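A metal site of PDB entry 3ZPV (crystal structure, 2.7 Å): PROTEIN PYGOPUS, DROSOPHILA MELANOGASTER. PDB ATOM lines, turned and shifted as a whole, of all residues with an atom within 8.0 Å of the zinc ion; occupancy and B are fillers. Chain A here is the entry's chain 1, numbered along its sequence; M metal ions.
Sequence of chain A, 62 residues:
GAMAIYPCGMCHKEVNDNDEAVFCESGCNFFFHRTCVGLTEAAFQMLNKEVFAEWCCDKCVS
The backbone carbonyl oxygen (O) of Glu 14 is in hydrogen-bond range of a ring nitrogen (NE2) of His 33 (3.0 Å).
NE2 of His 33 sits at hydrogen-bond distance from OD2 of Asp 19.
The side-chain sulfur (SG) of Cys 8 lies close to the backbone NH (N) of Met 10 (3.4 Å).
The backbone NH of Cys 8 lies within hydrogen-bond range of the backbone carbonyl oxygen of Lys 13 (2.9 Å).
The backbone NH of Lys 13 lies close to the side-chain sulfur of Cys 11 (3.5 Å).
Of the 18 residues printed, 4 come within 4 Å of the zinc ion.
The zinc ion is bound by a ring nitrogen (ND1) of His 33 (2.1 Å), the side-chain sulfur (SG) of Cys 36 (2.2 Å), the side-chain sulfur (SG) of Cys 8 (2.3 Å) and the side-chain sulfur (SG) of Cys 11 (2.3 Å).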
ATOM      1  N   PRO A   7     -10.096   6.824  16.630  1.00  0.00           N
ATOM      2  CA  PRO A   7      -9.163   5.729  16.524  1.00  0.00           C
ATOM      3  C   PRO A   7      -9.800   4.440  16.019  1.00  0.00           C
ATOM      4  O   PRO A   7     -10.969   4.154  16.287  1.00  0.00           O
ATOM      5  CB  PRO A   7      -8.694   5.553  17.955  1.00  0.00           C
ATOM      6  CG  PRO A   7      -9.874   5.934  18.773  1.00  0.00           C
ATOM      7  CD  PRO A   7     -10.622   6.970  18.000  1.00  0.00           C
ATOM      8  N   CYS A   8      -9.009   3.689  15.250  1.00  0.00           N
ATOM      9  CA  CYS A   8      -9.389   2.392  14.744  1.00  0.00           C
ATOM     10  C   CYS A   8      -9.648   1.505  15.944  1.00  0.00           C
ATOM     11  O   CYS A   8      -8.881   1.495  16.879  1.00  0.00           O
ATOM     12  CB  CYS A   8      -8.258   1.825  13.877  1.00  0.00           C
ATOM     13  SG  CYS A   8      -8.455   0.132  13.266  1.00  0.00           S
ATOM     14  N   GLY A   9     -10.736   0.736  15.901  1.00  0.00           N
ATOM     15  CA  GLY A   9     -11.010  -0.222  16.978  1.00  0.00           C
ATOM     16  C   GLY A   9     -10.024  -1.389  17.117  1.00  0.00           C
ATOM     17  O   GLY A   9     -10.021  -2.037  18.138  1.00  0.00           O
ATOM     18  N   MET A  10      -9.211  -1.639  16.091  1.00  0.00           N
ATOM     19  CA  MET A  10      -8.189  -2.675  16.083  1.00  0.00           C
ATOM     20  C   MET A  10      -6.845  -2.114  16.507  1.00  0.00           C
ATOM     21  O   MET A  10      -6.327  -2.462  17.556  1.00  0.00           O
ATOM     22  CB  MET A  10      -8.072  -3.270  14.662  1.00  0.00           C
ATOM     23  CG  MET A  10      -8.883  -4.551  14.430  1.00  0.00           C
ATOM     24  SD  MET A  10      -8.438  -5.957  15.480  1.00  0.00           S
ATOM     25  CE  MET A  10      -9.957  -6.094  16.467  1.00  0.00           C
ATOM     26  N   CYS A  11      -6.289  -1.228  15.682  1.00  0.00           N
ATOM     27  CA  CYS A  11      -4.910  -0.768  15.854  1.00  0.00           C
ATOM     28  C   CYS A  11      -4.793   0.516  16.703  1.00  0.00           C
ATOM     29  O   CYS A  11      -3.693   0.912  17.066  1.00  0.00           O
ATOM     30  CB  CYS A  11      -4.260  -0.534  14.489  1.00  0.00           C
ATOM     31  SG  CYS A  11      -4.792   0.967  13.616  1.00  0.00           S
ATOM     32  N   HIS A  12      -5.910   1.159  16.997  1.00  0.00           N
ATOM     33  CA  HIS A  12      -5.944   2.344  17.860  1.00  0.00           C
ATOM     34  C   HIS A  12      -5.293   3.583  17.299  1.00  0.00           C
ATOM     35  O   HIS A  12      -5.166   4.566  17.993  1.00  0.00           O
ATOM     36  CB  HIS A  12      -5.366   2.037  19.253  1.00  0.00           C
ATOM     37  CG  HIS A  12      -5.883   0.767  19.840  1.00  0.00           C
ATOM     38  ND1 HIS A  12      -7.235   0.603  20.141  1.00  0.00           N
ATOM     39  CD2 HIS A  12      -5.277  -0.403  20.146  1.00  0.00           C
ATOM     40  CE1 HIS A  12      -7.419  -0.618  20.618  1.00  0.00           C
ATOM     41  NE2 HIS A  12      -6.242  -1.241  20.638  1.00  0.00           N
ATOM     42  N   LYS A  13      -4.923   3.541  16.029  1.00  0.00           N
ATOM     43  CA  LYS A  13      -4.402   4.714  15.371  1.00  0.00           C
ATOM     44  C   LYS A  13      -5.498   5.462  14.678  1.00  0.00           C
ATOM     45  O   LYS A  13      -6.590   4.962  14.424  1.00  0.00           O
ATOM     46  CB  LYS A  13      -3.331   4.331  14.360  1.00  0.00           C
ATOM     47  CG  LYS A  13      -2.081   3.773  14.998  1.00  0.00           C
ATOM     48  CD  LYS A  13      -1.217   3.067  13.968  1.00  0.00           C
ATOM     49  CE  LYS A  13       0.201   2.905  14.492  1.00  0.00           C
ATOM     50  NZ  LYS A  13       1.103   2.323  13.459  1.00  0.00           N
ATOM     51  N   GLU A  14      -5.177   6.696  14.337  1.00  0.00           N
ATOM     52  CA  GLU A  14      -6.116   7.595  13.680  1.00  0.00           C
ATOM     53  C   GLU A  14      -6.735   7.005  12.392  1.00  0.00           C
ATOM     54  O   GLU A  14      -6.017   6.403  11.596  1.00  0.00           O
ATOM     55  CB  GLU A  14      -5.369   8.872  13.310  1.00  0.00           C
ATOM     56  CG  GLU A  14      -6.264  10.004  12.901  1.00  0.00           C
ATOM     57  CD  GLU A  14      -5.501  11.242  12.431  1.00  0.00           C
ATOM     58  OE1 GLU A  14      -4.285  11.337  12.724  1.00  0.00           O
ATOM     59  OE2 GLU A  14      -6.168  12.108  11.776  1.00  0.00           O
ATOM     60  N   VAL A  15      -8.043   7.183  12.235  1.00  0.00           N
ATOM     61  CA  VAL A  15      -8.706   6.943  10.988  1.00  0.00           C
ATOM     62  C   VAL A  15      -9.024   8.299  10.400  1.00  0.00           C
ATOM     63  O   VAL A  15      -9.863   9.006  10.938  1.00  0.00           O
ATOM     64  CB  VAL A  15     -10.038   6.193  11.176  1.00  0.00           C
ATOM     65  CG1 VAL A  15     -10.803   6.089   9.865  1.00  0.00           C
ATOM     66  CG2 VAL A  15      -9.806   4.800  11.710  1.00  0.00           C
ATOM     67  N   ASP A  19      -8.213   7.580   4.617  1.00  0.00           N
ATOM     68  CA  ASP A  19      -8.110   6.160   4.939  1.00  0.00           C
ATOM     69  C   ASP A  19      -9.307   5.421   4.320  1.00  0.00           C
ATOM     70  O   ASP A  19     -10.371   5.994   4.141  1.00  0.00           O
ATOM     71  CB  ASP A  19      -8.024   5.917   6.454  1.00  0.00           C
ATOM     72  CG  ASP A  19      -6.622   6.212   7.027  1.00  0.00           C
ATOM     73  OD1 ASP A  19      -5.632   6.134   6.281  1.00  0.00           O
ATOM     74  OD2 ASP A  19      -6.517   6.522   8.238  1.00  0.00           O
ATOM     75  N   GLU A  20      -9.105   4.164   3.959  1.00  0.00           N
ATOM     76  CA  GLU A  20     -10.184   3.299   3.554  1.00  0.00           C
ATOM     77  C   GLU A  20     -10.699   2.663   4.810  1.00  0.00           C
ATOM     78  O   GLU A  20      -9.996   1.858   5.438  1.00  0.00           O
ATOM     79  CB  GLU A  20      -9.706   2.213   2.601  1.00  0.00           C
ATOM     80  CG  GLU A  20      -9.178   2.696   1.254  1.00  0.00           C
ATOM     81  CD  GLU A  20      -8.927   1.576   0.257  1.00  0.00           C
ATOM     82  OE1 GLU A  20      -8.637   0.413   0.635  1.00  0.00           O
ATOM     83  OE2 GLU A  20      -9.019   1.870  -0.942  1.00  0.00           O
ATOM     84  N   PHE A  31     -14.851   3.362  14.363  1.00  0.00           N
ATOM     85  CA  PHE A  31     -14.328   3.259  13.018  1.00  0.00           C
ATOM     86  C   PHE A  31     -13.182   2.257  13.005  1.00  0.00           C
ATOM     87  O   PHE A  31     -12.567   2.024  14.015  1.00  0.00           O
ATOM     88  CB  PHE A  31     -13.816   4.607  12.530  1.00  0.00           C
ATOM     89  CG  PHE A  31     -14.892   5.601  12.280  1.00  0.00           C
ATOM     90  CD1 PHE A  31     -15.580   5.601  11.087  1.00  0.00           C
ATOM     91  CD2 PHE A  31     -15.249   6.513  13.270  1.00  0.00           C
ATOM     92  CE1 PHE A  31     -16.570   6.516  10.856  1.00  0.00           C
ATOM     93  CE2 PHE A  31     -16.234   7.417  13.045  1.00  0.00           C
ATOM     94  CZ  PHE A  31     -16.893   7.428  11.831  1.00  0.00           C
ATOM     95  N   PHE A  32     -12.923   1.686  11.851  1.00  0.00           N
ATOM     96  CA  PHE A  32     -11.837   0.731  11.651  1.00  0.00           C
ATOM     97  C   PHE A  32     -11.237   0.939  10.275  1.00  0.00           C
ATOM     98  O   PHE A  32     -11.942   1.201   9.323  1.00  0.00           O
ATOM     99  CB  PHE A  32     -12.370  -0.695  11.660  1.00  0.00           C
ATOM    100  CG  PHE A  32     -12.995  -1.149  12.943  1.00  0.00           C
ATOM    101  CD1 PHE A  32     -14.298  -0.826  13.242  1.00  0.00           C
ATOM    102  CD2 PHE A  32     -12.288  -1.949  13.832  1.00  0.00           C
ATOM    103  CE1 PHE A  32     -14.875  -1.265  14.420  1.00  0.00           C
ATOM    104  CE2 PHE A  32     -12.856  -2.413  15.021  1.00  0.00           C
ATOM    105  CZ  PHE A  32     -14.150  -2.082  15.311  1.00  0.00           C
ATOM    106  N   HIS A  33      -9.929   0.744  10.176  1.00  0.00           N
ATOM    107  CA  HIS A  33      -9.270   0.651   8.874  1.00  0.00           C
ATOM    108  C   HIS A  33      -9.709  -0.642   8.215  1.00  0.00           C
ATOM    109  O   HIS A  33      -9.784  -1.683   8.871  1.00  0.00           O
ATOM    110  CB  HIS A  33      -7.753   0.638   9.013  1.00  0.00           C
ATOM    111  CG  HIS A  33      -7.172   1.863   9.593  1.00  0.00           C
ATOM    112  ND1 HIS A  33      -6.573   1.882  10.836  1.00  0.00           N
ATOM    113  CD2 HIS A  33      -7.083   3.124   9.110  1.00  0.00           C
ATOM    114  CE1 HIS A  33      -6.145   3.106  11.103  1.00  0.00           C
ATOM    115  NE2 HIS A  33      -6.443   3.889  10.069  1.00  0.00           N
ATOM    116  N   ARG A  34      -9.947  -0.587   6.921  1.00  0.00           N
ATOM    117  CA  ARG A  34     -10.366  -1.762   6.190  1.00  0.00           C
ATOM    118  C   ARG A  34      -9.358  -2.916   6.340  1.00  0.00           C
ATOM    119  O   ARG A  34      -9.691  -4.085   6.577  1.00  0.00           O
ATOM    120  CB  ARG A  34     -10.531  -1.399   4.721  1.00  0.00           C
ATOM    121  CG  ARG A  34     -10.383  -2.601   3.786  1.00  0.00           C
ATOM    122  CD  ARG A  34     -10.457  -2.161   2.343  1.00  0.00           C
ATOM    123  NE  ARG A  34      -9.149  -1.937   1.757  1.00  0.00           N
ATOM    124  CZ  ARG A  34      -8.283  -2.889   1.462  1.00  0.00           C
ATOM    125  NH1 ARG A  34      -8.555  -4.171   1.724  1.00  0.00           N
ATOM    126  NH2 ARG A  34      -7.125  -2.565   0.908  1.00  0.00           N
ATOM    127  N   THR A  35      -8.108  -2.550   6.137  1.00  0.00           N
ATOM    128  CA  THR A  35      -7.013  -3.427   6.279  1.00  0.00           C
ATOM    129  C   THR A  35      -6.917  -4.138   7.639  1.00  0.00           C
ATOM    130  O   THR A  35      -6.641  -5.325   7.707  1.00  0.00           O
ATOM    131  CB  THR A  35      -5.821  -2.564   5.903  1.00  0.00           C
ATOM    132  OG1 THR A  35      -5.388  -2.951   4.624  1.00  0.00           O
ATOM    133  CG2 THR A  35      -4.750  -2.625   6.934  1.00  0.00           C
ATOM    134  N   CYS A  36      -7.132  -3.404   8.726  1.00  0.00           N
ATOM    135  CA  CYS A  36      -7.022  -3.952  10.083  1.00  0.00           C
ATOM    136  C   CYS A  36      -8.048  -5.026  10.389  1.00  0.00           C
ATOM    137  O   CYS A  36      -7.827  -5.852  11.257  1.00  0.00           O
ATOM    138  CB  CYS A  36      -7.142  -2.819  11.131  1.00  0.00           C
ATOM    139  SG  CYS A  36      -5.790  -1.630  11.170  1.00  0.00           S
ATOM    140  N   VAL A  37      -9.177  -5.001   9.698  1.00  0.00           N
ATOM    141  CA  VAL A  37     -10.249  -5.966  10.012  1.00  0.00           C
ATOM    142  C   VAL A  37     -10.295  -7.140   9.029  1.00  0.00           C
ATOM    143  O   VAL A  37     -11.035  -8.096   9.254  1.00  0.00           O
ATOM    144  CB  VAL A  37     -11.625  -5.289  10.076  1.00  0.00           C
ATOM    145  CG1 VAL A  37     -11.640  -4.303  11.217  1.00  0.00           C
ATOM    146  CG2 VAL A  37     -11.968  -4.583   8.773  1.00  0.00           C
HETATM  147 ZN    ZN M   1      -6.428   0.221  12.175  1.00  0.00          ZN
